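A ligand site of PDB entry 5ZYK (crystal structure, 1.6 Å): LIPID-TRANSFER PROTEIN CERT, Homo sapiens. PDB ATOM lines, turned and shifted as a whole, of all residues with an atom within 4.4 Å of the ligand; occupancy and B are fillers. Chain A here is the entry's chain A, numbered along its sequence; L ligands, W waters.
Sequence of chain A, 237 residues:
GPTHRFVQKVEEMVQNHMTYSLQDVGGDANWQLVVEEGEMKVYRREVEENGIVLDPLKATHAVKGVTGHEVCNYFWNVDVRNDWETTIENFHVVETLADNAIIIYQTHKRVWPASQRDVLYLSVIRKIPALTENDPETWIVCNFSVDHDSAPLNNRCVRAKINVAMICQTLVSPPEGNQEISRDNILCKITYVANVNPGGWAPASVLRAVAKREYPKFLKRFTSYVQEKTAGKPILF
CZ of Phe 75 touches O1 of the ligand (3.4 Å). Thr 87 touches the ligand. His 108 touches the ligand. Arg 117 touches the ligand. Tyr 121 touches the ligand (OH to C3, 3.7 Å). Ile 162 touches the ligand. Val 164 touches the ligand (CG1 to O1, 3.5 Å). CB of Pro 198 touches C10 of the ligand (3.9 Å). CD2 of Leu 207 touches C10 of the ligand (3.9 Å). Val 210 touches the ligand (CG1 to C22, 3.7 Å). Glu 214 touches the ligand. Tyr 215 touches the ligand (CZ to C24, 3.5 Å). Hydrophobic or aromatic side chains that line the ligand: Phe 75, His 108, Ile 162, Val 164, Tyr 192, Pro 198, Leu 207, Val 210 and Tyr 215. The nearest printed residue that does not touch the ligand is Val 196 (4.03 Å).
NE of Arg 117 is in hydrogen-bond range of O of Pro 198, at 2.8 Å. The backbone NH (N) of Asn 143 sits at hydrogen-bond distance from the backbone carbonyl oxygen (O) of Val 164 (2.8 Å). The backbone carbonyl oxygen of Phe 75 sits at hydrogen-bond distance from the guanidinium group of Arg 81 (3.2 Å). NE2 of His 108 sits at hydrogen-bond distance from NE2 of Gln 106, 2.9 Å away. The side-chain hydroxyl of Thr 87 sits at hydrogen-bond distance from a ring nitrogen (ND1) of His 108, 3.2 Å away. The side-chain hydroxyl (OH) of Tyr 121 is in hydrogen-bond range of the side-chain amide oxygen (OE1) of Gln 106 (2.7 Å). OH of Tyr 121 lies within hydrogen-bond range of NH2 of Arg 81, at 3.5 Å. The backbone carbonyl oxygen (O) of Arg 117 lies within hydrogen-bond range of the backbone NH (N) of His 108, at 2.9 Å.
OH of Tyr 192 lies within hydrogen-bond range of O1 of the ligand, at 2.8 Å. The side-chain amide nitrogen (ND2) of Asn 143 lies within hydrogen-bond range of an oxygen (O2) of the ligand (3.0 Å). NE2 of Gln 106 lies within hydrogen-bond range of O3 of the ligand, at 2.9 Å. O3 of the ligand is in hydrogen-bond range of OE1 of Glu 85, at 3.1 Å.
Water W2 bridges O3 of the ligand (2.9 Å) and OE2 of Glu 85 (3.1 Å). Water W1 bridges N1 of the ligand and ND1 of His 108.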
ATOM      1  N   PHE A  75     -11.882  11.497 -14.710  1.00  0.00           N
ATOM      2  CA  PHE A  75     -12.786  10.438 -15.193  1.00  0.00           C
ATOM      3  C   PHE A  75     -12.098   9.564 -16.246  1.00  0.00           C
ATOM      4  O   PHE A  75     -12.434   8.369 -16.322  1.00  0.00           O
ATOM      5  CB  PHE A  75     -14.032  11.146 -15.758  1.00  0.00           C
ATOM      6  CG  PHE A  75     -15.152  10.217 -16.176  1.00  0.00           C
ATOM      7  CD1 PHE A  75     -15.799   9.446 -15.217  1.00  0.00           C
ATOM      8  CD2 PHE A  75     -15.552  10.118 -17.495  1.00  0.00           C
ATOM      9  CE1 PHE A  75     -16.846   8.616 -15.585  1.00  0.00           C
ATOM     10  CE2 PHE A  75     -16.597   9.269 -17.879  1.00  0.00           C
ATOM     11  CZ  PHE A  75     -17.249   8.506 -16.918  1.00  0.00           C
ATOM     12  N   ARG A  81      -8.731   5.048 -11.499  1.00  0.00           N
ATOM     13  CA  ARG A  81     -10.037   4.438 -11.544  1.00  0.00           C
ATOM     14  C   ARG A  81     -10.421   3.812 -10.222  1.00  0.00           C
ATOM     15  O   ARG A  81     -11.554   4.011  -9.773  1.00  0.00           O
ATOM     16  CB  ARG A  81     -10.068   3.287 -12.553  1.00  0.00           C
ATOM     17  CG  ARG A  81     -11.479   2.837 -12.934  1.00  0.00           C
ATOM     18  CD  ARG A  81     -12.400   3.880 -13.560  1.00  0.00           C
ATOM     19  NE  ARG A  81     -11.802   4.756 -14.560  1.00  0.00           N
ATOM     20  CZ  ARG A  81     -11.821   4.530 -15.873  1.00  0.00           C
ATOM     21  NH1 ARG A  81     -11.316   5.447 -16.691  1.00  0.00           N
ATOM     22  NH2 ARG A  81     -12.325   3.409 -16.351  1.00  0.00           N
ATOM     23  N   TRP A  84     -12.107   5.683  -7.287  1.00  0.00           N
ATOM     24  CA  TRP A  84     -13.506   6.111  -7.192  1.00  0.00           C
ATOM     25  C   TRP A  84     -14.524   5.053  -7.651  1.00  0.00           C
ATOM     26  O   TRP A  84     -15.680   5.152  -7.253  1.00  0.00           O
ATOM     27  CB  TRP A  84     -13.757   7.465  -7.914  1.00  0.00           C
ATOM     28  CG  TRP A  84     -13.400   7.458  -9.366  1.00  0.00           C
ATOM     29  CD1 TRP A  84     -12.214   7.821  -9.916  1.00  0.00           C
ATOM     30  CD2 TRP A  84     -14.241   7.067 -10.462  1.00  0.00           C
ATOM     31  NE1 TRP A  84     -12.251   7.676 -11.288  1.00  0.00           N
ATOM     32  CE2 TRP A  84     -13.489   7.213 -11.645  1.00  0.00           C
ATOM     33  CE3 TRP A  84     -15.558   6.576 -10.544  1.00  0.00           C
ATOM     34  CZ2 TRP A  84     -13.981   6.903 -12.901  1.00  0.00           C
ATOM     35  CZ3 TRP A  84     -16.044   6.295 -11.802  1.00  0.00           C
ATOM     36  CH2 TRP A  84     -15.278   6.430 -12.957  1.00  0.00           C
ATOM     37  N   GLU A  85     -14.132   4.113  -8.552  1.00  0.00           N
ATOM     38  CA  GLU A  85     -15.078   3.108  -9.059  1.00  0.00           C
ATOM     39  C   GLU A  85     -15.425   2.113  -7.965  1.00  0.00           C
ATOM     40  O   GLU A  85     -14.500   1.680  -7.268  1.00  0.00           O
ATOM     41  CB  GLU A  85     -14.320   2.198 -10.041  1.00  0.00           C
ATOM     42  CG  GLU A  85     -14.153   2.769 -11.429  1.00  0.00           C
ATOM     43  CD  GLU A  85     -15.391   2.629 -12.284  1.00  0.00           C
ATOM     44  OE1 GLU A  85     -15.243   2.527 -13.499  1.00  0.00           O
ATOM     45  OE2 GLU A  85     -16.477   2.652 -11.732  1.00  0.00           O
ATOM     46  N   THR A  87     -17.949  -0.528  -8.825  1.00  0.00           N
ATOM     47  CA  THR A  87     -18.671  -1.665  -9.377  1.00  0.00           C
ATOM     48  C   THR A  87     -17.840  -2.505 -10.339  1.00  0.00           C
ATOM     49  O   THR A  87     -18.419  -3.316 -11.046  1.00  0.00           O
ATOM     50  CB  THR A  87     -19.930  -1.185 -10.126  1.00  0.00           C
ATOM     51  OG1 THR A  87     -19.586  -0.511 -11.329  1.00  0.00           O
ATOM     52  CG2 THR A  87     -20.815  -0.332  -9.243  1.00  0.00           C
ATOM     53  N   ILE A  88     -16.543  -2.222 -10.477  1.00  0.00           N
ATOM     54  CA  ILE A  88     -15.702  -2.928 -11.441  1.00  0.00           C
ATOM     55  C   ILE A  88     -15.047  -4.087 -10.720  1.00  0.00           C
ATOM     56  O   ILE A  88     -14.581  -3.945  -9.587  1.00  0.00           O
ATOM     57  CB  ILE A  88     -14.584  -1.990 -11.930  1.00  0.00           C
ATOM     58  CG1 ILE A  88     -15.176  -0.824 -12.692  1.00  0.00           C
ATOM     59  CG2 ILE A  88     -13.637  -2.718 -12.871  1.00  0.00           C
ATOM     60  CD1 ILE A  88     -15.893  -1.256 -13.865  1.00  0.00           C
ATOM     61  N   GLN A 106     -13.625  -4.356 -19.424  1.00  0.00           N
ATOM     62  CA  GLN A 106     -13.843  -4.381 -17.964  1.00  0.00           C
ATOM     63  C   GLN A 106     -15.016  -5.315 -17.650  1.00  0.00           C
ATOM     64  O   GLN A 106     -15.893  -5.531 -18.504  1.00  0.00           O
ATOM     65  CB  GLN A 106     -14.027  -3.018 -17.262  1.00  0.00           C
ATOM     66  CG  GLN A 106     -15.353  -2.335 -17.687  1.00  0.00           C
ATOM     67  CD  GLN A 106     -15.349  -0.874 -17.315  1.00  0.00           C
ATOM     68  OE1 GLN A 106     -14.324  -0.202 -17.329  1.00  0.00           O
ATOM     69  NE2 GLN A 106     -16.563  -0.371 -17.044  1.00  0.00           N
ATOM     70  N   HIS A 108     -18.081  -5.981 -14.688  1.00  0.00           N
ATOM     71  CA  HIS A 108     -18.779  -5.393 -13.554  1.00  0.00           C
ATOM     72  C   HIS A 108     -19.119  -6.437 -12.527  1.00  0.00           C
ATOM     73  O   HIS A 108     -19.393  -7.582 -12.860  1.00  0.00           O
ATOM     74  CB  HIS A 108     -20.038  -4.671 -14.031  1.00  0.00           C
ATOM     75  CG  HIS A 108     -19.633  -3.411 -14.721  1.00  0.00           C
ATOM     76  ND1 HIS A 108     -19.441  -2.201 -14.021  1.00  0.00           N
ATOM     77  CD2 HIS A 108     -19.201  -3.211 -15.986  1.00  0.00           C
ATOM     78  CE1 HIS A 108     -19.049  -1.284 -14.889  1.00  0.00           C
ATOM     79  NE2 HIS A 108     -18.889  -1.878 -16.078  1.00  0.00           N
ATOM     80  N   VAL A 111     -24.887  -8.406 -10.746  1.00  0.00           N
ATOM     81  CA  VAL A 111     -26.165  -7.931 -10.210  1.00  0.00           C
ATOM     82  C   VAL A 111     -27.112  -9.142 -10.236  1.00  0.00           C
ATOM     83  O   VAL A 111     -27.611  -9.538 -11.278  1.00  0.00           O
ATOM     84  CB  VAL A 111     -26.730  -6.785 -11.052  1.00  0.00           C
ATOM     85  CG1 VAL A 111     -28.116  -6.369 -10.574  1.00  0.00           C
ATOM     86  CG2 VAL A 111     -25.736  -5.610 -11.090  1.00  0.00           C
ATOM     87  N   ARG A 117     -21.939  -8.988 -16.261  1.00  0.00           N
ATOM     88  CA  ARG A 117     -21.693  -8.310 -17.533  1.00  0.00           C
ATOM     89  C   ARG A 117     -20.211  -7.922 -17.674  1.00  0.00           C
ATOM     90  O   ARG A 117     -19.550  -7.515 -16.706  1.00  0.00           O
ATOM     91  CB  ARG A 117     -22.547  -7.023 -17.668  1.00  0.00           C
ATOM     92  CG  ARG A 117     -23.849  -7.197 -18.438  1.00  0.00           C
ATOM     93  CD  ARG A 117     -24.757  -8.338 -17.921  1.00  0.00           C
ATOM     94  NE  ARG A 117     -25.926  -8.445 -18.809  1.00  0.00           N
ATOM     95  CZ  ARG A 117     -26.878  -9.369 -18.633  1.00  0.00           C
ATOM     96  NH1 ARG A 117     -26.802 -10.234 -17.612  1.00  0.00           N
ATOM     97  NH2 ARG A 117     -27.880  -9.437 -19.513  1.00  0.00           N
ATOM     98  N   TYR A 121     -14.906  -1.051 -24.697  1.00  0.00           N
ATOM     99  CA  TYR A 121     -15.258   0.283 -25.182  1.00  0.00           C
ATOM    100  C   TYR A 121     -14.056   1.166 -25.470  1.00  0.00           C
ATOM    101  O   TYR A 121     -12.996   1.001 -24.882  1.00  0.00           O
ATOM    102  CB  TYR A 121     -16.174   1.045 -24.200  1.00  0.00           C
ATOM    103  CG  TYR A 121     -15.640   1.285 -22.789  1.00  0.00           C
ATOM    104  CD1 TYR A 121     -15.592   0.258 -21.838  1.00  0.00           C
ATOM    105  CD2 TYR A 121     -15.074   2.502 -22.398  1.00  0.00           C
ATOM    106  CE1 TYR A 121     -15.082   0.458 -20.553  1.00  0.00           C
ATOM    107  CE2 TYR A 121     -14.559   2.735 -21.124  1.00  0.00           C
ATOM    108  CZ  TYR A 121     -14.569   1.711 -20.191  1.00  0.00           C
ATOM    109  OH  TYR A 121     -14.094   1.936 -18.940  1.00  0.00           O
ATOM    110  N   ASN A 143     -17.307   7.345 -23.659  1.00  0.00           N
ATOM    111  CA  ASN A 143     -16.978   5.927 -23.554  1.00  0.00           C
ATOM    112  C   ASN A 143     -18.026   5.205 -24.381  1.00  0.00           C
ATOM    113  O   ASN A 143     -19.210   5.208 -24.022  1.00  0.00           O
ATOM    114  CB  ASN A 143     -17.083   5.465 -22.093  1.00  0.00           C
ATOM    115  CG  ASN A 143     -15.991   6.050 -21.215  1.00  0.00           C
ATOM    116  OD1 ASN A 143     -14.943   6.464 -21.715  1.00  0.00           O
ATOM    117  ND2 ASN A 143     -16.205   6.155 -19.913  1.00  0.00           N
ATOM    118  N   ILE A 162     -22.326   0.079 -24.312  1.00  0.00           N
ATOM    119  CA  ILE A 162     -22.510   1.377 -23.641  1.00  0.00           C
ATOM    120  C   ILE A 162     -22.267   2.527 -24.581  1.00  0.00           C
ATOM    121  O   ILE A 162     -21.516   2.436 -25.575  1.00  0.00           O
ATOM    122  CB  ILE A 162     -21.623   1.529 -22.409  1.00  0.00           C
ATOM    123  CG1 ILE A 162     -20.129   1.674 -22.750  1.00  0.00           C
ATOM    124  CG2 ILE A 162     -21.899   0.386 -21.445  1.00  0.00           C
ATOM    125  CD1 ILE A 162     -19.247   2.047 -21.545  1.00  0.00           C
ATOM    126  N   VAL A 164     -21.660   6.396 -23.194  1.00  0.00           N
ATOM    127  CA  VAL A 164     -21.666   7.237 -22.007  1.00  0.00           C
ATOM    128  C   VAL A 164     -20.872   8.504 -22.337  1.00  0.00           C
ATOM    129  O   VAL A 164     -19.839   8.498 -23.059  1.00  0.00           O
ATOM    130  CB  VAL A 164     -20.939   6.517 -20.840  1.00  0.00           C
ATOM    131  CG1 VAL A 164     -20.580   7.473 -19.687  1.00  0.00           C
ATOM    132  CG2 VAL A 164     -21.783   5.331 -20.317  1.00  0.00           C
ATOM    133  N   TYR A 192     -24.127  14.378 -17.555  1.00  0.00           N
ATOM    134  CA  TYR A 192     -23.660  13.006 -17.648  1.00  0.00           C
ATOM    135  C   TYR A 192     -24.777  12.193 -18.303  1.00  0.00           C
ATOM    136  O   TYR A 192     -25.923  12.243 -17.847  1.00  0.00           O
ATOM    137  CB  TYR A 192     -23.327  12.443 -16.258  1.00  0.00           C
ATOM    138  CG  TYR A 192     -23.061  10.963 -16.254  1.00  0.00           C
ATOM    139  CD1 TYR A 192     -21.798  10.507 -16.564  1.00  0.00           C
ATOM    140  CD2 TYR A 192     -24.040  10.031 -15.954  1.00  0.00           C
ATOM    141  CE1 TYR A 192     -21.533   9.140 -16.557  1.00  0.00           C
ATOM    142  CE2 TYR A 192     -23.794   8.648 -15.983  1.00  0.00           C
ATOM    143  CZ  TYR A 192     -22.524   8.198 -16.292  1.00  0.00           C
ATOM    144  OH  TYR A 192     -22.275   6.822 -16.298  1.00  0.00           O
ATOM    145  N   VAL A 196     -27.091   2.322 -21.705  1.00  0.00           N
ATOM    146  CA  VAL A 196     -26.529   1.000 -21.429  1.00  0.00           C
ATOM    147  C   VAL A 196     -27.479  -0.053 -21.951  1.00  0.00           C
ATOM    148  O   VAL A 196     -28.671  -0.078 -21.643  1.00  0.00           O
ATOM    149  CB  VAL A 196     -26.299   0.811 -19.933  1.00  0.00           C
ATOM    150  CG1 VAL A 196     -25.790  -0.634 -19.662  1.00  0.00           C
ATOM    151  CG2 VAL A 196     -25.289   1.805 -19.409  1.00  0.00           C
ATOM    152  N   PRO A 198     -27.914  -3.958 -21.658  1.00  0.00           N
ATOM    153  CA  PRO A 198     -27.425  -5.095 -20.896  1.00  0.00           C
ATOM    154  C   PRO A 198     -27.034  -6.285 -21.768  1.00  0.00           C
ATOM    155  O   PRO A 198     -26.365  -7.169 -21.245  1.00  0.00           O
ATOM    156  CB  PRO A 198     -28.597  -5.488 -19.978  1.00  0.00           C
ATOM    157  CG  PRO A 198     -29.440  -4.207 -19.875  1.00  0.00           C
ATOM    158  CD  PRO A 198     -29.288  -3.562 -21.249  1.00  0.00           C
ATOM    159  N   LEU A 207     -32.875  -4.168 -12.414  1.00  0.00           N
ATOM    160  CA  LEU A 207     -31.972  -3.250 -13.113  1.00  0.00           C
ATOM    161  C   LEU A 207     -32.365  -1.811 -12.793  1.00  0.00           C
ATOM    162  O   LEU A 207     -31.523  -0.932 -12.594  1.00  0.00           O
ATOM    163  CB  LEU A 207     -31.992  -3.436 -14.634  1.00  0.00           C
ATOM    164  CG  LEU A 207     -31.202  -4.624 -15.189  1.00  0.00           C
ATOM    165  CD1 LEU A 207     -31.199  -4.529 -16.708  1.00  0.00           C
ATOM    166  CD2 LEU A 207     -29.793  -4.690 -14.619  1.00  0.00           C
ATOM    167  N   VAL A 210     -31.274  -0.828  -9.283  1.00  0.00           N
ATOM    168  CA  VAL A 210     -29.806  -0.686  -9.196  1.00  0.00           C
ATOM    169  C   VAL A 210     -29.383   0.639  -9.814  1.00  0.00           C
ATOM    170  O   VAL A 210     -28.606   1.396  -9.212  1.00  0.00           O
ATOM    171  CB  VAL A 210     -29.098  -1.884  -9.857  1.00  0.00           C
ATOM    172  CG1 VAL A 210     -27.642  -1.586 -10.129  1.00  0.00           C
ATOM    173  CG2 VAL A 210     -29.305  -3.098  -8.958  1.00  0.00           C
ATOM    174  N   ALA A 211     -29.991   0.983 -10.963  1.00  0.00           N
ATOM    175  CA  ALA A 211     -29.599   2.232 -11.604  1.00  0.00           C
ATOM    176  C   ALA A 211     -29.970   3.399 -10.697  1.00  0.00           C
ATOM    177  O   ALA A 211     -29.196   4.368 -10.574  1.00  0.00           O
ATOM    178  CB  ALA A 211     -30.251   2.383 -12.957  1.00  0.00           C
ATOM    179  N   GLU A 214     -27.324   3.423  -7.929  1.00  0.00           N
ATOM    180  CA  GLU A 214     -25.884   3.483  -8.200  1.00  0.00           C
ATOM    181  C   GLU A 214     -25.484   4.730  -9.020  1.00  0.00           C
ATOM    182  O   GLU A 214     -24.322   5.188  -8.893  1.00  0.00           O
ATOM    183  CB  GLU A 214     -25.430   2.249  -8.993  1.00  0.00           C
ATOM    184  CG  GLU A 214     -25.544   0.978  -8.144  1.00  0.00           C
ATOM    185  CD  GLU A 214     -24.563   0.893  -6.987  1.00  0.00           C
ATOM    186  OE1 GLU A 214     -23.453   1.473  -7.083  1.00  0.00           O
ATOM    187  OE2 GLU A 214     -24.899   0.215  -5.953  1.00  0.00           O
ATOM    188  N   TYR A 215     -26.363   5.253  -9.899  1.00  0.00           N
ATOM    189  CA  TYR A 215     -25.928   6.459 -10.628  1.00  0.00           C
ATOM    190  C   TYR A 215     -25.745   7.630  -9.668  1.00  0.00           C
ATOM    191  O   TYR A 215     -24.739   8.323  -9.790  1.00  0.00           O
ATOM    192  CB  TYR A 215     -26.893   6.785 -11.796  1.00  0.00           C
ATOM    193  CG  TYR A 215     -26.674   5.894 -12.992  1.00  0.00           C
ATOM    194  CD1 TYR A 215     -25.478   5.994 -13.727  1.00  0.00           C
ATOM    195  CD2 TYR A 215     -27.656   5.015 -13.418  1.00  0.00           C
ATOM    196  CE1 TYR A 215     -25.281   5.279 -14.890  1.00  0.00           C
ATOM    197  CE2 TYR A 215     -27.427   4.227 -14.562  1.00  0.00           C
ATOM    198  CZ  TYR A 215     -26.239   4.347 -15.260  1.00  0.00           C
ATOM    199  OH  TYR A 215     -26.052   3.564 -16.391  1.00  0.00           O
HETATM  200  C1  LIG L   1     -25.930  -3.808 -17.176  1.00  0.00           C
HETATM  201  C2  LIG L   1     -21.016   3.527 -15.978  1.00  0.00           C
HETATM  202  C3  LIG L   1     -16.379   3.586 -16.510  1.00  0.00           C
HETATM  203  C4  LIG L   1     -17.423   4.664 -16.088  1.00  0.00           C
HETATM  204  C5  LIG L   1     -19.977   3.473 -16.893  1.00  0.00           C
HETATM  205  C6  LIG L   1     -22.658   0.188 -16.430  1.00  0.00           C
HETATM  206  C7  LIG L   1     -23.924   0.382 -15.823  1.00  0.00           C
HETATM  207  C8  LIG L   1     -26.170  -0.356 -14.917  1.00  0.00           C
HETATM  208  C9  LIG L   1     -24.854  -0.647 -15.586  1.00  0.00           C
HETATM  209  N1  LIG L   1     -23.873   0.237 -12.721  1.00  0.00           N
HETATM  210  C10 LIG L   1     -26.521  -5.168 -16.701  1.00  0.00           C
HETATM  211  C11 LIG L   1     -24.544  -1.976 -16.039  1.00  0.00           C
HETATM  212  C12 LIG L   1     -23.255  -2.174 -16.626  1.00  0.00           C
HETATM  213  C13 LIG L   1     -21.768   1.320 -16.604  1.00  0.00           C
HETATM  214  O1  LIG L   1     -19.629   6.076 -16.577  1.00  0.00           O
HETATM  215  S1  LIG L   1     -18.908   4.861 -17.118  1.00  0.00           S
HETATM  216  O2  LIG L   1     -18.454   4.748 -18.458  1.00  0.00           O
HETATM  217  O3  LIG L   1     -16.924   2.366 -16.056  1.00  0.00           O
HETATM  218  C14 LIG L   1     -19.765   2.293 -17.675  1.00  0.00           C
HETATM  219  C15 LIG L   1     -20.704   1.230 -17.468  1.00  0.00           C
HETATM  220  C16 LIG L   1     -21.924   2.480 -15.798  1.00  0.00           C
HETATM  221  C17 LIG L   1     -22.325  -1.138 -16.883  1.00  0.00           C
HETATM  222  C18 LIG L   1     -25.524  -3.139 -15.851  1.00  0.00           C
HETATM  223  C19 LIG L   1     -25.008  -4.300 -14.950  1.00  0.00           C
HETATM  224  C20 LIG L   1     -25.956  -5.485 -15.334  1.00  0.00           C
HETATM  225  C21 LIG L   1     -26.199   0.472 -13.618  1.00  0.00           C
HETATM  226  C22 LIG L   1     -26.626  -0.977 -13.613  1.00  0.00           C
HETATM  227  C23 LIG L   1     -24.940   1.048 -12.976  1.00  0.00           C
HETATM  228  C24 LIG L   1     -24.799   2.443 -12.731  1.00  0.00           C
HETATM  229  C25 LIG L   1     -23.625   2.995 -12.199  1.00  0.00           C
HETATM  230  C26 LIG L   1     -22.503   2.168 -11.930  1.00  0.00           C
HETATM  231  C27 LIG L   1     -22.715   0.814 -12.265  1.00  0.00           C
HETATM  232  O   HOH W   1     -22.703  -2.373 -12.965  1.00  0.00           O
HETATM  233  O   HOH W   2     -18.715   2.404 -13.814  1.00  0.00           O
